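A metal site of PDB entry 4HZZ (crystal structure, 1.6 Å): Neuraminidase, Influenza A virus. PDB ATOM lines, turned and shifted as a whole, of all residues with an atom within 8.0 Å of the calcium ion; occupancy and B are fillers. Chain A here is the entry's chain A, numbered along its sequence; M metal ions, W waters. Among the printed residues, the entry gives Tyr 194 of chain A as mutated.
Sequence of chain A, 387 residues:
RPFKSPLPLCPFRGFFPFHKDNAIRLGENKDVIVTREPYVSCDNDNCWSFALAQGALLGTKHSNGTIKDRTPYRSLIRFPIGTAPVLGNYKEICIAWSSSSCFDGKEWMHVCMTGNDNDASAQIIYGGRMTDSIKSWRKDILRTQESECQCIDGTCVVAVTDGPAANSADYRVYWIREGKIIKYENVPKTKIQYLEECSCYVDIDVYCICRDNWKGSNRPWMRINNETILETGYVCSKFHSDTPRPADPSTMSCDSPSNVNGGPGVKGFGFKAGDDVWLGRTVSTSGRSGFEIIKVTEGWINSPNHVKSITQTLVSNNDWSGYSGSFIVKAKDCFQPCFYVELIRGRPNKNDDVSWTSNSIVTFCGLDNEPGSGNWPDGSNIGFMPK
The calcium ion is bound by O of Asp 212 (2.3 Å), O of Gly 216 (2.3 Å), OD2 of Asp 242 (2.4 Å), water W1 (2.4 Å) and O of Gly 262 (2.4 Å).
O of Thr 243 lies close to N of Gly 265.
The guanidinium group of Arg 219 lies within salt-bridge range of the side-chain carboxylate of Asp 242 (3.3 Å).
The backbone NH of Asp 242 sits at hydrogen-bond distance from the backbone carbonyl oxygen of Ser 217.
OD1 of Asp 242 lies within hydrogen-bond range of N of Val 266 (2.8 Å).
The side-chain carboxylate (OD2) of Asp 212 is in hydrogen-bond range of the side-chain hydroxyl (OH) of Tyr 234, 2.7 Å away.
The side-chain carboxylate of Asp 212 lies within hydrogen-bond range of the backbone NH of Gly 216 (3.1 Å).
The guanidinium group (NH2) of Arg 245 lies within hydrogen-bond range of the backbone carbonyl oxygen (O) of Asp 242 (3.0 Å).
The backbone carbonyl oxygen of Gly 265 is in hydrogen-bond range of the guanidinium group of Arg 211 (3.2 Å).
Water W1 bridges O of Pro 244 (2.7 Å) and O of Asn 261 (2.8 Å).
Merely in contact with the calcium ion: Gly 265 (3.8 Å).
Five residues have an atom within 4 Å of the calcium ion: Asp 212, Gly 216, Asp 242, Gly 262 and Gly 265.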
ATOM      1  N   TYR A 194      12.441  -6.329 -29.863  1.00  0.00           N
ATOM      2  CA  TYR A 194      13.547  -5.665 -29.148  1.00  0.00           C
ATOM      3  C   TYR A 194      13.756  -6.365 -27.819  1.00  0.00           C
ATOM      4  O   TYR A 194      12.802  -6.703 -27.140  1.00  0.00           O
ATOM      5  CB  TYR A 194      13.248  -4.181 -28.936  1.00  0.00           C
ATOM      6  CG  TYR A 194      12.927  -3.476 -30.231  1.00  0.00           C
ATOM      7  CD1 TYR A 194      13.915  -2.845 -30.970  1.00  0.00           C
ATOM      8  CD2 TYR A 194      11.637  -3.482 -30.734  1.00  0.00           C
ATOM      9  CE1 TYR A 194      13.630  -2.221 -32.170  1.00  0.00           C
ATOM     10  CE2 TYR A 194      11.338  -2.858 -31.933  1.00  0.00           C
ATOM     11  CZ  TYR A 194      12.334  -2.228 -32.651  1.00  0.00           C
ATOM     12  OH  TYR A 194      12.036  -1.624 -33.851  1.00  0.00           O
ATOM     13  N   CYS A 210      12.631  -9.413 -20.284  1.00  0.00           N
ATOM     14  CA  CYS A 210      13.557  -8.372 -20.729  1.00  0.00           C
ATOM     15  C   CYS A 210      12.896  -7.023 -21.006  1.00  0.00           C
ATOM     16  O   CYS A 210      11.776  -6.752 -20.562  1.00  0.00           O
ATOM     17  CB  CYS A 210      14.328  -8.891 -21.955  1.00  0.00           C
ATOM     18  SG  CYS A 210      14.825 -10.645 -21.800  1.00  0.00           S
ATOM     19  N   ARG A 211      13.613  -6.155 -21.707  1.00  0.00           N
ATOM     20  CA  ARG A 211      13.172  -4.787 -21.957  1.00  0.00           C
ATOM     21  C   ARG A 211      13.089  -4.528 -23.456  1.00  0.00           C
ATOM     22  O   ARG A 211      14.109  -4.538 -24.138  1.00  0.00           O
ATOM     23  CB  ARG A 211      14.170  -3.816 -21.309  1.00  0.00           C
ATOM     24  CG  ARG A 211      14.053  -2.342 -21.664  1.00  0.00           C
ATOM     25  CD  ARG A 211      15.275  -1.579 -21.108  1.00  0.00           C
ATOM     26  NE  ARG A 211      15.327  -0.166 -21.542  1.00  0.00           N
ATOM     27  CZ  ARG A 211      16.173   0.721 -21.038  1.00  0.00           C
ATOM     28  NH1 ARG A 211      17.051   0.369 -20.106  1.00  0.00           N
ATOM     29  NH2 ARG A 211      16.140   1.981 -21.478  1.00  0.00           N
ATOM     30  N   ASP A 212      11.874  -4.310 -23.958  1.00  0.00           N
ATOM     31  CA  ASP A 212      11.737  -3.826 -25.316  1.00  0.00           C
ATOM     32  C   ASP A 212      11.872  -2.311 -25.206  1.00  0.00           C
ATOM     33  O   ASP A 212      11.056  -1.660 -24.570  1.00  0.00           O
ATOM     34  CB  ASP A 212      10.379  -4.264 -25.895  1.00  0.00           C
ATOM     35  CG  ASP A 212      10.102  -3.665 -27.265  1.00  0.00           C
ATOM     36  OD1 ASP A 212      10.472  -2.513 -27.492  1.00  0.00           O
ATOM     37  OD2 ASP A 212       9.453  -4.357 -28.079  1.00  0.00           O
ATOM     38  N   ASN A 213      12.928  -1.751 -25.780  1.00  0.00           N
ATOM     39  CA  ASN A 213      13.197  -0.331 -25.607  1.00  0.00           C
ATOM     40  C   ASN A 213      12.635   0.549 -26.719  1.00  0.00           C
ATOM     41  O   ASN A 213      12.961   1.717 -26.809  1.00  0.00           O
ATOM     42  CB  ASN A 213      14.688  -0.050 -25.405  1.00  0.00           C
ATOM     43  CG  ASN A 213      15.526  -0.346 -26.652  1.00  0.00           C
ATOM     44  OD1 ASN A 213      16.503   0.364 -26.921  1.00  0.00           O
ATOM     45  ND2 ASN A 213      15.158  -1.367 -27.392  1.00  0.00           N
ATOM     46  N   TRP A 214      11.774  -0.011 -27.556  1.00  0.00           N
ATOM     47  CA  TRP A 214      11.342   0.717 -28.747  1.00  0.00           C
ATOM     48  C   TRP A 214       9.830   0.706 -28.992  1.00  0.00           C
ATOM     49  O   TRP A 214       9.214   1.764 -29.192  1.00  0.00           O
ATOM     50  CB  TRP A 214      12.086   0.176 -29.973  1.00  0.00           C
ATOM     51  CG  TRP A 214      12.135   1.125 -31.131  1.00  0.00           C
ATOM     52  CD1 TRP A 214      11.487   1.002 -32.330  1.00  0.00           C
ATOM     53  CD2 TRP A 214      12.871   2.350 -31.196  1.00  0.00           C
ATOM     54  NE1 TRP A 214      11.786   2.074 -33.143  1.00  0.00           N
ATOM     55  CE2 TRP A 214      12.628   2.918 -32.469  1.00  0.00           C
ATOM     56  CE3 TRP A 214      13.714   3.029 -30.313  1.00  0.00           C
ATOM     57  CZ2 TRP A 214      13.200   4.123 -32.874  1.00  0.00           C
ATOM     58  CZ3 TRP A 214      14.281   4.234 -30.711  1.00  0.00           C
ATOM     59  CH2 TRP A 214      14.010   4.770 -31.984  1.00  0.00           C
ATOM     60  N   LYS A 215       9.233  -0.482 -28.976  1.00  0.00           N
ATOM     61  CA  LYS A 215       7.833  -0.625 -29.384  1.00  0.00           C
ATOM     62  C   LYS A 215       6.906  -1.210 -28.329  1.00  0.00           C
ATOM     63  O   LYS A 215       5.685  -1.180 -28.508  1.00  0.00           O
ATOM     64  CB  LYS A 215       7.741  -1.503 -30.637  1.00  0.00           C
ATOM     65  CG  LYS A 215       8.376  -0.917 -31.892  1.00  0.00           C
ATOM     66  CD  LYS A 215       7.839   0.468 -32.216  1.00  0.00           C
ATOM     67  CE  LYS A 215       8.418   0.983 -33.541  1.00  0.00           C
ATOM     68  NZ  LYS A 215       8.037   2.394 -33.828  1.00  0.00           N
ATOM     69  N   GLY A 216       7.452  -1.770 -27.252  1.00  0.00           N
ATOM     70  CA  GLY A 216       6.626  -2.547 -26.347  1.00  0.00           C
ATOM     71  C   GLY A 216       6.610  -2.059 -24.906  1.00  0.00           C
ATOM     72  O   GLY A 216       7.655  -1.997 -24.271  1.00  0.00           O
ATOM     73  N   SER A 217       5.425  -1.711 -24.408  1.00  0.00           N
ATOM     74  CA  SER A 217       5.246  -1.410 -22.993  1.00  0.00           C
ATOM     75  C   SER A 217       5.055  -2.707 -22.203  1.00  0.00           C
ATOM     76  O   SER A 217       5.152  -2.720 -20.962  1.00  0.00           O
ATOM     77  CB  SER A 217       4.052  -0.476 -22.766  1.00  0.00           C
ATOM     78  OG  SER A 217       2.899  -0.983 -23.419  1.00  0.00           O
ATOM     79  N   ASN A 218       4.747  -3.786 -22.919  1.00  0.00           N
ATOM     80  CA  ASN A 218       4.768  -5.129 -22.359  1.00  0.00           C
ATOM     81  C   ASN A 218       6.161  -5.715 -22.545  1.00  0.00           C
ATOM     82  O   ASN A 218       6.897  -5.302 -23.447  1.00  0.00           O
ATOM     83  CB  ASN A 218       3.696  -6.023 -23.016  1.00  0.00           C
ATOM     84  CG  ASN A 218       3.772  -6.036 -24.549  1.00  0.00           C
ATOM     85  OD1 ASN A 218       4.335  -5.137 -25.172  1.00  0.00           O
ATOM     86  ND2 ASN A 218       3.228  -7.099 -25.141  1.00  0.00           N
ATOM     87  N   ARG A 219       6.551  -6.637 -21.675  1.00  0.00           N
ATOM     88  CA  ARG A 219       7.919  -7.157 -21.717  1.00  0.00           C
ATOM     89  C   ARG A 219       8.095  -8.412 -22.557  1.00  0.00           C
ATOM     90  O   ARG A 219       7.306  -9.350 -22.456  1.00  0.00           O
ATOM     91  CB  ARG A 219       8.418  -7.436 -20.300  1.00  0.00           C
ATOM     92  CG  ARG A 219       8.602  -6.175 -19.469  1.00  0.00           C
ATOM     93  CD  ARG A 219       9.447  -6.445 -18.223  1.00  0.00           C
ATOM     94  NE  ARG A 219       9.647  -5.232 -17.422  1.00  0.00           N
ATOM     95  CZ  ARG A 219      10.518  -4.266 -17.731  1.00  0.00           C
ATOM     96  NH1 ARG A 219      11.284  -4.388 -18.829  1.00  0.00           N
ATOM     97  NH2 ARG A 219      10.609  -3.187 -16.970  1.00  0.00           N
ATOM     98  N   PRO A 220       9.175  -8.448 -23.348  1.00  0.00           N
ATOM     99  CA  PRO A 220       9.515  -9.647 -24.116  1.00  0.00           C
ATOM    100  C   PRO A 220      10.132 -10.681 -23.208  1.00  0.00           C
ATOM    101  O   PRO A 220      10.672 -10.330 -22.149  1.00  0.00           O
ATOM    102  CB  PRO A 220      10.568  -9.128 -25.115  1.00  0.00           C
ATOM    103  CG  PRO A 220      11.213  -7.984 -24.398  1.00  0.00           C
ATOM    104  CD  PRO A 220      10.122  -7.349 -23.580  1.00  0.00           C
ATOM    105  N   TYR A 234       5.923 -12.182 -25.786  1.00  0.00           N
ATOM    106  CA  TYR A 234       5.782 -11.036 -24.893  1.00  0.00           C
ATOM    107  C   TYR A 234       4.851 -11.463 -23.763  1.00  0.00           C
ATOM    108  O   TYR A 234       4.012 -12.347 -23.935  1.00  0.00           O
ATOM    109  CB  TYR A 234       5.228  -9.804 -25.609  1.00  0.00           C
ATOM    110  CG  TYR A 234       6.257  -9.030 -26.410  1.00  0.00           C
ATOM    111  CD1 TYR A 234       6.671  -9.495 -27.648  1.00  0.00           C
ATOM    112  CD2 TYR A 234       6.798  -7.845 -25.922  1.00  0.00           C
ATOM    113  CE1 TYR A 234       7.614  -8.797 -28.384  1.00  0.00           C
ATOM    114  CE2 TYR A 234       7.742  -7.147 -26.643  1.00  0.00           C
ATOM    115  CZ  TYR A 234       8.142  -7.623 -27.881  1.00  0.00           C
ATOM    116  OH  TYR A 234       9.079  -6.935 -28.609  1.00  0.00           O
ATOM    117  N   SER A 241       4.167  -3.865 -17.727  1.00  0.00           N
ATOM    118  CA  SER A 241       5.133  -3.666 -16.640  1.00  0.00           C
ATOM    119  C   SER A 241       6.439  -2.970 -16.988  1.00  0.00           C
ATOM    120  O   SER A 241       7.337  -2.889 -16.134  1.00  0.00           O
ATOM    121  CB  SER A 241       5.421  -4.991 -15.929  1.00  0.00           C
ATOM    122  OG  SER A 241       6.014  -5.927 -16.802  1.00  0.00           O
ATOM    123  N   ASP A 242       6.569  -2.457 -18.208  1.00  0.00           N
ATOM    124  CA  ASP A 242       7.707  -1.609 -18.539  1.00  0.00           C
ATOM    125  C   ASP A 242       7.382  -0.160 -18.149  1.00  0.00           C
ATOM    126  O   ASP A 242       6.308   0.122 -17.636  1.00  0.00           O
ATOM    127  CB  ASP A 242       8.058  -1.711 -20.043  1.00  0.00           C
ATOM    128  CG  ASP A 242       9.534  -1.419 -20.328  1.00  0.00           C
ATOM    129  OD1 ASP A 242      10.262  -0.977 -19.417  1.00  0.00           O
ATOM    130  OD2 ASP A 242       9.984  -1.645 -21.464  1.00  0.00           O
ATOM    131  N   THR A 243       8.339   0.738 -18.357  1.00  0.00           N
ATOM    132  CA  THR A 243       8.158   2.166 -18.094  1.00  0.00           C
ATOM    133  C   THR A 243       8.782   2.949 -19.253  1.00  0.00           C
ATOM    134  O   THR A 243       9.966   2.827 -19.505  1.00  0.00           O
ATOM    135  CB  THR A 243       8.874   2.610 -16.800  1.00  0.00           C
ATOM    136  OG1 THR A 243       8.455   1.776 -15.715  1.00  0.00           O
ATOM    137  CG2 THR A 243       8.532   4.069 -16.465  1.00  0.00           C
ATOM    138  N   PRO A 244       7.992   3.761 -19.952  1.00  0.00           N
ATOM    139  CA  PRO A 244       6.564   4.073 -19.720  1.00  0.00           C
ATOM    140  C   PRO A 244       5.647   2.951 -20.155  1.00  0.00           C
ATOM    141  O   PRO A 244       6.080   1.931 -20.704  1.00  0.00           O
ATOM    142  CB  PRO A 244       6.343   5.294 -20.606  1.00  0.00           C
ATOM    143  CG  PRO A 244       7.295   5.091 -21.757  1.00  0.00           C
ATOM    144  CD  PRO A 244       8.527   4.451 -21.130  1.00  0.00           C
ATOM    145  N   ARG A 245       4.353   3.129 -19.890  1.00  0.00           N
ATOM    146  CA  ARG A 245       3.347   2.151 -20.261  1.00  0.00           C
ATOM    147  C   ARG A 245       1.984   2.809 -20.139  1.00  0.00           C
ATOM    148  O   ARG A 245       1.844   3.850 -19.496  1.00  0.00           O
ATOM    149  CB  ARG A 245       3.413   0.933 -19.354  1.00  0.00           C
ATOM    150  CG  ARG A 245       3.156   1.270 -17.899  1.00  0.00           C
ATOM    151  CD  ARG A 245       3.107   0.037 -17.029  1.00  0.00           C
ATOM    152  NE  ARG A 245       2.767   0.393 -15.662  1.00  0.00           N
ATOM    153  CZ  ARG A 245       3.656   0.742 -14.732  1.00  0.00           C
ATOM    154  NH1 ARG A 245       3.233   1.068 -13.524  1.00  0.00           N
ATOM    155  NH2 ARG A 245       4.968   0.756 -15.008  1.00  0.00           N
ATOM    156  N   PRO A 257       4.964  -6.726 -29.514  1.00  0.00           N
ATOM    157  CA  PRO A 257       4.969  -5.543 -28.648  1.00  0.00           C
ATOM    158  C   PRO A 257       3.617  -4.831 -28.702  1.00  0.00           C
ATOM    159  O   PRO A 257       2.910  -4.900 -29.720  1.00  0.00           O
ATOM    160  CB  PRO A 257       6.049  -4.641 -29.273  1.00  0.00           C
ATOM    161  CG  PRO A 257       6.210  -5.154 -30.677  1.00  0.00           C
ATOM    162  CD  PRO A 257       5.953  -6.619 -30.610  1.00  0.00           C
ATOM    163  N   SER A 258       3.277  -4.129 -27.626  1.00  0.00           N
ATOM    164  CA  SER A 258       2.022  -3.385 -27.548  1.00  0.00           C
ATOM    165  C   SER A 258       1.905  -2.276 -28.590  1.00  0.00           C
ATOM    166  O   SER A 258       0.802  -1.837 -28.922  1.00  0.00           O
ATOM    167  CB  SER A 258       1.890  -2.760 -26.164  1.00  0.00           C
ATOM    168  OG  SER A 258       2.864  -1.749 -26.010  1.00  0.00           O
ATOM    169  N   VAL A 260       2.617   0.779 -28.129  1.00  0.00           N
ATOM    170  CA  VAL A 260       2.325   2.054 -27.475  1.00  0.00           C
ATOM    171  C   VAL A 260       3.307   2.272 -26.331  1.00  0.00           C
ATOM    172  O   VAL A 260       3.725   1.315 -25.696  1.00  0.00           O
ATOM    173  CB  VAL A 260       0.888   2.098 -26.915  1.00  0.00           C
ATOM    174  CG1 VAL A 260      -0.120   2.328 -28.027  1.00  0.00           C
ATOM    175  CG2 VAL A 260       0.553   0.825 -26.147  1.00  0.00           C
ATOM    176  N   ASN A 261       3.685   3.535 -26.096  1.00  0.00           N
ATOM    177  CA  ASN A 261       4.589   3.872 -25.003  1.00  0.00           C
ATOM    178  C   ASN A 261       5.806   2.964 -24.990  1.00  0.00           C
ATOM    179  O   ASN A 261       6.234   2.489 -23.949  1.00  0.00           O
ATOM    180  CB  ASN A 261       3.865   3.750 -23.664  1.00  0.00           C
ATOM    181  CG  ASN A 261       2.625   4.615 -23.593  1.00  0.00           C
ATOM    182  OD1 ASN A 261       2.725   5.841 -23.615  1.00  0.00           O
ATOM    183  ND2 ASN A 261       1.468   3.981 -23.484  1.00  0.00           N
ATOM    184  N   GLY A 262       6.375   2.734 -26.167  1.00  0.00           N
ATOM    185  CA  GLY A 262       7.392   1.721 -26.316  1.00  0.00           C
ATOM    186  C   GLY A 262       8.753   1.998 -25.691  1.00  0.00           C
ATOM    187  O   GLY A 262       9.429   1.067 -25.279  1.00  0.00           O
ATOM    188  N   GLY A 263       9.166   3.256 -25.642  1.00  0.00           N
ATOM    189  CA  GLY A 263      10.517   3.567 -25.199  1.00  0.00           C
ATOM    190  C   GLY A 263      10.525   4.676 -24.172  1.00  0.00           C
ATOM    191  O   GLY A 263       9.567   5.433 -24.080  1.00  0.00           O
ATOM    192  N   PRO A 264      11.622   4.788 -23.418  1.00  0.00           N
ATOM    193  CA  PRO A 264      12.843   3.974 -23.573  1.00  0.00           C
ATOM    194  C   PRO A 264      12.821   2.635 -22.834  1.00  0.00           C
ATOM    195  O   PRO A 264      13.728   1.819 -23.046  1.00  0.00           O
ATOM    196  CB  PRO A 264      13.913   4.868 -22.944  1.00  0.00           C
ATOM    197  CG  PRO A 264      13.176   5.593 -21.864  1.00  0.00           C
ATOM    198  CD  PRO A 264      11.819   5.897 -22.463  1.00  0.00           C
ATOM    199  N   GLY A 265      11.827   2.413 -21.981  1.00  0.00           N
ATOM    200  CA  GLY A 265      11.795   1.222 -21.161  1.00  0.00           C
ATOM    201  C   GLY A 265      12.747   1.328 -19.997  1.00  0.00           C
ATOM    202  O   GLY A 265      13.461   2.318 -19.839  1.00  0.00           O
ATOM    203  N   VAL A 266      12.745   0.289 -19.168  1.00  0.00           N
ATOM    204  CA  VAL A 266      13.642   0.193 -18.013  1.00  0.00           C
ATOM    205  C   VAL A 266      13.882  -1.293 -17.792  1.00  0.00           C
ATOM    206  O   VAL A 266      13.013  -2.106 -18.081  1.00  0.00           O
ATOM    207  CB  VAL A 266      13.027   0.889 -16.755  1.00  0.00           C
ATOM    208  CG1 VAL A 266      11.801   0.133 -16.242  1.00  0.00           C
ATOM    209  CG2 VAL A 266      14.060   1.051 -15.636  1.00  0.00           C
HETATM  210 CA    CA M   1       9.353  -0.577 -23.482  1.00  0.00          CA
HETATM  211  O   HOH W   1       8.138   1.197 -22.367  1.00  0.00           O
